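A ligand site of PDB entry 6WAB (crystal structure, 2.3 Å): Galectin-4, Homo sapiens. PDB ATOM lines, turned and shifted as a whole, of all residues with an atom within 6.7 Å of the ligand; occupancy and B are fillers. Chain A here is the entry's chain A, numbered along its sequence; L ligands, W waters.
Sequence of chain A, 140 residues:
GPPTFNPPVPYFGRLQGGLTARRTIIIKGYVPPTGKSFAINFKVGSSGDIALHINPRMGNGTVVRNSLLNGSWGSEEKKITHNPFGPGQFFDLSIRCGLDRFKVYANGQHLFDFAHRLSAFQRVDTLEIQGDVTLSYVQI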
ATOM      1  N   SER A  37     -31.236 -17.207  19.258  1.00  0.00           N
ATOM      2  CA  SER A  37     -30.416 -18.235  19.921  1.00  0.00           C
ATOM      3  C   SER A  37     -30.996 -19.609  19.619  1.00  0.00           C
ATOM      4  O   SER A  37     -32.226 -19.732  19.583  1.00  0.00           O
ATOM      5  CB  SER A  37     -30.296 -17.959  21.430  1.00  0.00           C
ATOM      6  OG  SER A  37     -31.010 -18.900  22.199  1.00  0.00           O
ATOM      7  N   PHE A  38     -30.131 -20.587  19.391  1.00  0.00           N
ATOM      8  CA  PHE A  38     -30.533 -22.003  19.431  1.00  0.00           C
ATOM      9  C   PHE A  38     -29.564 -22.790  20.287  1.00  0.00           C
ATOM     10  O   PHE A  38     -28.483 -22.312  20.589  1.00  0.00           O
ATOM     11  CB  PHE A  38     -30.620 -22.600  18.036  1.00  0.00           C
ATOM     12  CG  PHE A  38     -29.331 -22.785  17.306  1.00  0.00           C
ATOM     13  CD1 PHE A  38     -28.638 -23.979  17.384  1.00  0.00           C
ATOM     14  CD2 PHE A  38     -28.842 -21.786  16.467  1.00  0.00           C
ATOM     15  CE1 PHE A  38     -27.493 -24.173  16.644  1.00  0.00           C
ATOM     16  CE2 PHE A  38     -27.680 -21.977  15.757  1.00  0.00           C
ATOM     17  CZ  PHE A  38     -27.020 -23.177  15.821  1.00  0.00           C
ATOM     18  N   ALA A  39     -30.004 -23.983  20.649  1.00  0.00           N
ATOM     19  CA  ALA A  39     -29.269 -24.891  21.543  1.00  0.00           C
ATOM     20  C   ALA A  39     -29.225 -26.265  20.923  1.00  0.00           C
ATOM     21  O   ALA A  39     -30.218 -26.698  20.386  1.00  0.00           O
ATOM     22  CB  ALA A  39     -29.917 -24.978  22.907  1.00  0.00           C
ATOM     23  N   ASN A  41     -28.186 -29.920  22.644  1.00  0.00           N
ATOM     24  CA  ASN A  41     -28.002 -30.607  23.948  1.00  0.00           C
ATOM     25  C   ASN A  41     -27.734 -32.098  23.724  1.00  0.00           C
ATOM     26  O   ASN A  41     -28.575 -32.774  23.137  1.00  0.00           O
ATOM     27  CB  ASN A  41     -29.213 -30.529  24.890  1.00  0.00           C
ATOM     28  CG  ASN A  41     -29.508 -29.130  25.386  1.00  0.00           C
ATOM     29  OD1 ASN A  41     -28.594 -28.339  25.626  1.00  0.00           O
ATOM     30  ND2 ASN A  41     -30.795 -28.822  25.474  1.00  0.00           N
ATOM     31  N   ILE A  50     -27.162 -32.422  31.112  1.00  0.00           N
ATOM     32  CA  ILE A  50     -26.580 -32.076  29.781  1.00  0.00           C
ATOM     33  C   ILE A  50     -25.045 -32.122  29.873  1.00  0.00           C
ATOM     34  O   ILE A  50     -24.418 -31.204  30.432  1.00  0.00           O
ATOM     35  CB  ILE A  50     -27.162 -30.744  29.265  1.00  0.00           C
ATOM     36  CG1 ILE A  50     -28.690 -30.817  29.175  1.00  0.00           C
ATOM     37  CG2 ILE A  50     -26.525 -30.376  27.928  1.00  0.00           C
ATOM     38  CD1 ILE A  50     -29.393 -29.495  28.917  1.00  0.00           C
ATOM     39  N   HIS A  53     -23.800 -28.712  26.114  1.00  0.00           N
ATOM     40  CA  HIS A  53     -24.794 -27.712  25.660  1.00  0.00           C
ATOM     41  C   HIS A  53     -24.056 -26.695  24.816  1.00  0.00           C
ATOM     42  O   HIS A  53     -23.128 -26.114  25.330  1.00  0.00           O
ATOM     43  CB  HIS A  53     -25.455 -27.002  26.853  1.00  0.00           C
ATOM     44  CG  HIS A  53     -26.345 -25.856  26.505  1.00  0.00           C
ATOM     45  ND1 HIS A  53     -27.659 -26.044  26.096  1.00  0.00           N
ATOM     46  CD2 HIS A  53     -26.136 -24.529  26.531  1.00  0.00           C
ATOM     47  CE1 HIS A  53     -28.205 -24.859  25.921  1.00  0.00           C
ATOM     48  NE2 HIS A  53     -27.285 -23.919  26.164  1.00  0.00           N
ATOM     49  N   ILE A  54     -24.490 -26.514  23.565  1.00  0.00           N
ATOM     50  CA  ILE A  54     -23.885 -25.569  22.577  1.00  0.00           C
ATOM     51  C   ILE A  54     -24.968 -24.531  22.265  1.00  0.00           C
ATOM     52  O   ILE A  54     -26.073 -24.904  21.746  1.00  0.00           O
ATOM     53  CB  ILE A  54     -23.435 -26.300  21.300  1.00  0.00           C
ATOM     54  CG1 ILE A  54     -22.639 -27.577  21.575  1.00  0.00           C
ATOM     55  CG2 ILE A  54     -22.672 -25.337  20.388  1.00  0.00           C
ATOM     56  CD1 ILE A  54     -22.669 -28.550  20.383  1.00  0.00           C
ATOM     57  N   ASN A  55     -24.690 -23.269  22.584  1.00  0.00           N
ATOM     58  CA  ASN A  55     -25.695 -22.184  22.522  1.00  0.00           C
ATOM     59  C   ASN A  55     -25.126 -21.033  21.703  1.00  0.00           C
ATOM     60  O   ASN A  55     -24.535 -20.120  22.270  1.00  0.00           O
ATOM     61  CB  ASN A  55     -26.036 -21.709  23.942  1.00  0.00           C
ATOM     62  CG  ASN A  55     -27.228 -20.788  23.929  1.00  0.00           C
ATOM     63  OD1 ASN A  55     -27.403 -20.039  24.860  1.00  0.00           O
ATOM     64  ND2 ASN A  55     -28.003 -20.819  22.848  1.00  0.00           N
ATOM     65  N   PRO A  56     -25.209 -21.081  20.365  1.00  0.00           N
ATOM     66  CA  PRO A  56     -25.018 -19.891  19.539  1.00  0.00           C
ATOM     67  C   PRO A  56     -26.085 -18.844  19.824  1.00  0.00           C
ATOM     68  O   PRO A  56     -27.278 -19.157  19.704  1.00  0.00           O
ATOM     69  CB  PRO A  56     -25.154 -20.459  18.115  1.00  0.00           C
ATOM     70  CG  PRO A  56     -24.651 -21.864  18.269  1.00  0.00           C
ATOM     71  CD  PRO A  56     -25.362 -22.288  19.534  1.00  0.00           C
ATOM     72  N   ARG A  57     -25.626 -17.631  20.177  1.00  0.00           N
ATOM     73  CA  ARG A  57     -26.435 -16.448  20.495  1.00  0.00           C
ATOM     74  C   ARG A  57     -26.102 -15.338  19.508  1.00  0.00           C
ATOM     75  O   ARG A  57     -24.961 -14.787  19.600  1.00  0.00           O
ATOM     76  CB  ARG A  57     -26.112 -16.016  21.911  1.00  0.00           C
ATOM     77  CG  ARG A  57     -26.397 -17.107  22.922  1.00  0.00           C
ATOM     78  CD  ARG A  57     -26.056 -16.662  24.327  1.00  0.00           C
ATOM     79  NE  ARG A  57     -26.297 -17.704  25.328  1.00  0.00           N
ATOM     80  CZ  ARG A  57     -25.930 -17.615  26.592  1.00  0.00           C
ATOM     81  NH1 ARG A  57     -25.297 -16.536  27.013  1.00  0.00           N
ATOM     82  NH2 ARG A  57     -26.186 -18.613  27.424  1.00  0.00           N
ATOM     83  N   VAL A  64     -21.673 -20.468  23.071  1.00  0.00           N
ATOM     84  CA  VAL A  64     -21.529 -20.783  24.516  1.00  0.00           C
ATOM     85  C   VAL A  64     -21.594 -22.303  24.694  1.00  0.00           C
ATOM     86  O   VAL A  64     -22.573 -22.938  24.276  1.00  0.00           O
ATOM     87  CB  VAL A  64     -22.560 -20.011  25.375  1.00  0.00           C
ATOM     88  CG1 VAL A  64     -22.196 -20.015  26.850  1.00  0.00           C
ATOM     89  CG2 VAL A  64     -22.699 -18.576  24.888  1.00  0.00           C
ATOM     90  N   ARG A  65     -20.549 -22.857  25.316  1.00  0.00           N
ATOM     91  CA  ARG A  65     -20.486 -24.286  25.699  1.00  0.00           C
ATOM     92  C   ARG A  65     -20.537 -24.419  27.225  1.00  0.00           C
ATOM     93  O   ARG A  65     -19.807 -23.682  27.943  1.00  0.00           O
ATOM     94  CB  ARG A  65     -19.231 -24.921  25.099  1.00  0.00           C
ATOM     95  CG  ARG A  65     -19.259 -25.007  23.573  1.00  0.00           C
ATOM     96  CD  ARG A  65     -18.628 -23.774  22.944  1.00  0.00           C
ATOM     97  NE  ARG A  65     -17.206 -23.795  23.265  1.00  0.00           N
ATOM     98  CZ  ARG A  65     -16.309 -22.847  22.972  1.00  0.00           C
ATOM     99  NH1 ARG A  65     -16.681 -21.713  22.374  1.00  0.00           N
ATOM    100  NH2 ARG A  65     -15.040 -23.047  23.304  1.00  0.00           N
ATOM    101  N   ASN A  66     -21.343 -25.349  27.705  1.00  0.00           N
ATOM    102  CA  ASN A  66     -21.462 -25.663  29.147  1.00  0.00           C
ATOM    103  C   ASN A  66     -22.011 -27.095  29.286  1.00  0.00           C
ATOM    104  O   ASN A  66     -22.262 -27.790  28.235  1.00  0.00           O
ATOM    105  CB  ASN A  66     -22.337 -24.623  29.883  1.00  0.00           C
ATOM    106  CG  ASN A  66     -21.865 -24.314  31.292  1.00  0.00           C
ATOM    107  OD1 ASN A  66     -21.044 -25.039  31.859  1.00  0.00           O
ATOM    108  ND2 ASN A  66     -22.344 -23.221  31.863  1.00  0.00           N
ATOM    109  N   SER A  67     -22.128 -27.517  30.551  1.00  0.00           N
ATOM    110  CA  SER A  67     -22.837 -28.720  31.028  1.00  0.00           C
ATOM    111  C   SER A  67     -23.849 -28.326  32.119  1.00  0.00           C
ATOM    112  O   SER A  67     -23.574 -27.396  32.874  1.00  0.00           O
ATOM    113  CB  SER A  67     -21.835 -29.727  31.538  1.00  0.00           C
ATOM    114  OG  SER A  67     -20.784 -29.903  30.591  1.00  0.00           O
ATOM    115  N   TRP A  73     -25.303 -25.257  36.187  1.00  0.00           N
ATOM    116  CA  TRP A  73     -24.579 -24.779  34.969  1.00  0.00           C
ATOM    117  C   TRP A  73     -23.132 -24.568  35.367  1.00  0.00           C
ATOM    118  O   TRP A  73     -22.913 -23.812  36.317  1.00  0.00           O
ATOM    119  CB  TRP A  73     -25.178 -23.474  34.425  1.00  0.00           C
ATOM    120  CG  TRP A  73     -26.430 -23.654  33.612  1.00  0.00           C
ATOM    121  CD1 TRP A  73     -27.654 -23.104  33.828  1.00  0.00           C
ATOM    122  CD2 TRP A  73     -26.569 -24.446  32.405  1.00  0.00           C
ATOM    123  NE1 TRP A  73     -28.540 -23.508  32.866  1.00  0.00           N
ATOM    124  CE2 TRP A  73     -27.909 -24.328  31.981  1.00  0.00           C
ATOM    125  CE3 TRP A  73     -25.692 -25.221  31.648  1.00  0.00           C
ATOM    126  CZ2 TRP A  73     -28.380 -24.959  30.843  1.00  0.00           C
ATOM    127  CZ3 TRP A  73     -26.151 -25.846  30.516  1.00  0.00           C
ATOM    128  CH2 TRP A  73     -27.484 -25.698  30.118  1.00  0.00           C
ATOM    129  N   GLY A  74     -22.202 -25.258  34.685  1.00  0.00           N
ATOM    130  CA  GLY A  74     -20.768 -25.173  34.995  1.00  0.00           C
ATOM    131  C   GLY A  74     -20.193 -23.868  34.465  1.00  0.00           C
ATOM    132  O   GLY A  74     -20.976 -22.939  34.183  1.00  0.00           O
ATOM    133  N   SER A  75     -18.865 -23.782  34.375  1.00  0.00           N
ATOM    134  CA  SER A  75     -18.110 -22.677  33.741  1.00  0.00           C
ATOM    135  C   SER A  75     -18.394 -22.663  32.219  1.00  0.00           C
ATOM    136  O   SER A  75     -18.387 -23.741  31.564  1.00  0.00           O
ATOM    137  CB  SER A  75     -16.649 -22.783  34.020  1.00  0.00           C
ATOM    138  OG  SER A  75     -16.444 -22.974  35.411  1.00  0.00           O
ATOM    139  N   GLU A  76     -18.649 -21.480  31.682  1.00  0.00           N
ATOM    140  CA  GLU A  76     -18.977 -21.282  30.261  1.00  0.00           C
ATOM    141  C   GLU A  76     -17.687 -21.309  29.469  1.00  0.00           C
ATOM    142  O   GLU A  76     -16.771 -20.685  29.905  1.00  0.00           O
ATOM    143  CB  GLU A  76     -19.711 -19.956  30.107  1.00  0.00           C
ATOM    144  CG  GLU A  76     -21.105 -20.039  30.649  1.00  0.00           C
ATOM    145  CD  GLU A  76     -22.015 -18.885  30.252  1.00  0.00           C
ATOM    146  OE1 GLU A  76     -23.255 -19.025  30.397  1.00  0.00           O
ATOM    147  OE2 GLU A  76     -21.484 -17.855  29.814  1.00  0.00           O
ATOM    148  N   GLU A 128     -30.819 -33.125  21.380  1.00  0.00           N
ATOM    149  CA  GLU A 128     -31.938 -32.157  21.322  1.00  0.00           C
ATOM    150  C   GLU A 128     -31.408 -30.877  20.686  1.00  0.00           C
ATOM    151  O   GLU A 128     -30.280 -30.478  20.975  1.00  0.00           O
ATOM    152  CB  GLU A 128     -32.593 -32.115  22.710  1.00  0.00           C
ATOM    153  CG  GLU A 128     -32.686 -30.783  23.376  1.00  0.00           C
ATOM    154  CD  GLU A 128     -32.902 -30.925  24.884  1.00  0.00           C
ATOM    155  OE1 GLU A 128     -32.878 -29.893  25.565  1.00  0.00           O
ATOM    156  OE2 GLU A 128     -33.118 -32.050  25.364  1.00  0.00           O
ATOM    157  N   GLN A 130     -33.088 -27.120  19.691  1.00  0.00           N
ATOM    158  CA  GLN A 130     -34.232 -26.234  19.975  1.00  0.00           C
ATOM    159  C   GLN A 130     -33.851 -24.809  19.558  1.00  0.00           C
ATOM    160  O   GLN A 130     -32.636 -24.531  19.548  1.00  0.00           O
ATOM    161  CB  GLN A 130     -34.511 -26.263  21.482  1.00  0.00           C
ATOM    162  CG  GLN A 130     -34.593 -27.655  22.065  1.00  0.00           C
ATOM    163  CD  GLN A 130     -35.266 -27.616  23.423  1.00  0.00           C
ATOM    164  OE1 GLN A 130     -36.443 -27.938  23.543  1.00  0.00           O
ATOM    165  NE2 GLN A 130     -34.536 -27.166  24.437  1.00  0.00           N
ATOM    166  N   GLY A 131     -34.854 -23.958  19.337  1.00  0.00           N
ATOM    167  CA  GLY A 131     -34.704 -22.502  19.211  1.00  0.00           C
ATOM    168  C   GLY A 131     -34.643 -22.064  17.763  1.00  0.00           C
ATOM    169  O   GLY A 131     -35.291 -22.710  16.928  1.00  0.00           O
ATOM    170  N   ASP A 132     -33.874 -21.029  17.468  1.00  0.00           N
ATOM    171  CA  ASP A 132     -33.914 -20.266  16.201  1.00  0.00           C
ATOM    172  C   ASP A 132     -32.919 -20.913  15.231  1.00  0.00           C
ATOM    173  O   ASP A 132     -31.817 -20.348  14.998  1.00  0.00           O
ATOM    174  CB  ASP A 132     -33.737 -18.783  16.491  1.00  0.00           C
ATOM    175  CG  ASP A 132     -34.626 -18.304  17.637  1.00  0.00           C
ATOM    176  OD1 ASP A 132     -35.756 -18.891  17.795  1.00  0.00           O
ATOM    177  OD2 ASP A 132     -34.212 -17.369  18.365  1.00  0.00           O
HETATM  178  C1  LIG L   1     -24.678 -19.429  36.213  1.00  0.00           C
HETATM  179  C2  LIG L   1     -23.527 -19.804  36.944  1.00  0.00           C
HETATM  180  C3  LIG L   1     -22.384 -20.252  36.297  1.00  0.00           C
HETATM  181  F1  LIG L   1     -21.084 -20.630  37.103  1.00  0.00           F
HETATM  182  C4  LIG L   1     -22.428 -20.316  34.898  1.00  0.00           C
HETATM  183  C5  LIG L   1     -23.580 -19.936  34.180  1.00  0.00           C
HETATM  184  C6  LIG L   1     -24.729 -19.481  34.817  1.00  0.00           C
HETATM  185  C7  LIG L   1     -25.866 -19.164  34.170  1.00  0.00           C
HETATM  186  C8  LIG L   1     -26.042 -19.009  32.832  1.00  0.00           C
HETATM  187  N1  LIG L   1     -27.058 -18.986  34.785  1.00  0.00           N
HETATM  188  N2  LIG L   1     -27.968 -18.704  33.810  1.00  0.00           N
HETATM  189  N3  LIG L   1     -27.316 -18.724  32.588  1.00  0.00           N
HETATM  190  C9  LIG L   1     -27.857 -18.543  31.265  1.00  0.00           C
HETATM  191  C10 LIG L   1     -27.959 -20.001  30.762  1.00  0.00           C
HETATM  192  C11 LIG L   1     -28.987 -20.295  29.691  1.00  0.00           C
HETATM  193  O1  LIG L   1     -30.305 -20.280  30.106  1.00  0.00           O
HETATM  194  O2  LIG L   1     -26.655 -20.215  30.174  1.00  0.00           O
HETATM  195  C12 LIG L   1     -26.419 -21.578  29.830  1.00  0.00           C
HETATM  196  C13 LIG L   1     -24.956 -21.933  29.424  1.00  0.00           C
HETATM  197  O3  LIG L   1     -24.057 -21.380  30.404  1.00  0.00           O
HETATM  198  C14 LIG L   1     -27.419 -21.981  28.726  1.00  0.00           C
HETATM  199  O4  LIG L   1     -27.221 -21.195  27.473  1.00  0.00           O
HETATM  200  C15 LIG L   1     -28.820 -21.766  29.303  1.00  0.00           C
HETATM  201  N4  LIG L   1     -29.821 -22.210  28.284  1.00  0.00           N
HETATM  202  C16 LIG L   1     -30.153 -21.727  27.085  1.00  0.00           C
HETATM  203  N5  LIG L   1     -30.533 -23.250  28.507  1.00  0.00           N
HETATM  204  N6  LIG L   1     -31.304 -23.446  27.452  1.00  0.00           N
HETATM  205  C17 LIG L   1     -31.078 -22.518  26.571  1.00  0.00           C
HETATM  206  C18 LIG L   1     -31.698 -22.468  25.372  1.00  0.00           C
HETATM  207  C19 LIG L   1     -31.382 -21.505  24.389  1.00  0.00           C
HETATM  208  C20 LIG L   1     -32.053 -21.547  23.148  1.00  0.00           C
HETATM  209  C21 LIG L   1     -33.032 -22.519  22.916  1.00  0.00           C
HETATM  210  C22 LIG L   1     -33.328 -23.500  23.876  1.00  0.00           C
HETATM  211  C23 LIG L   1     -32.659 -23.478  25.086  1.00  0.00           C
HETATM  212  O   HOH W   1     -31.377 -21.078  32.851  1.00  0.00           O
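OE1 of Glu 76 is in hydrogen-bond range of O3 of the ligand (2.5 Å).
An oxygen (O4) of the ligand sits at hydrogen-bond distance from the guanidinium group (NH2) of Arg 57 (2.8 Å).
O4 of the ligand lies within hydrogen-bond range of OD1 of Asn 55, at 2.9 Å.
The side-chain amide nitrogen of Asn 66 lies within hydrogen-bond range of an oxygen (O3) of the ligand.
A ring nitrogen (NE2) of His 53 sits at hydrogen-bond distance from an oxygen (O4) of the ligand.
ND2 of Asn 55 sits at hydrogen-bond distance from O of Phe 38 (2.8 Å).
The backbone carbonyl oxygen (O) of Val 64 is in hydrogen-bond range of the backbone NH (N) of Asn 55.
The side-chain amide nitrogen (ND2) of Asn 66 lies within hydrogen-bond range of the backbone carbonyl oxygen (O) of Gly 74 (2.7 Å).
The backbone carbonyl oxygen of Ser 37 is in hydrogen-bond range of the backbone NH of Asp 132 (3.0 Å).
N of Gly 74 sits at hydrogen-bond distance from O of Ser 67 (3.1 Å).
The backbone NH of Ala 39 sits at hydrogen-bond distance from the backbone carbonyl oxygen of Gln 130 (2.9 Å).
NE2 of Gln 130 sits at hydrogen-bond distance from OE1 of Glu 128 (3.4 Å).
The backbone NH (N) of Phe 38 is in hydrogen-bond range of the backbone carbonyl oxygen (O) of Pro 56 (3.2 Å).
Residues that only touch the ligand: Ser 37 (3.0 Å), Gly 74 (3.1 Å), Trp 73 (3.6 Å), Ala 39 (3.8 Å), Gln 130 (3.8 Å) and Phe 38 (3.99 Å).
11 residues have an atom within 4 Å of the ligand: Ser 37, Phe 38, Ala 39, His 53, Asn 55, Arg 57, Asn 66, Trp 73, Gly 74, Glu 76 and Gln 130.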
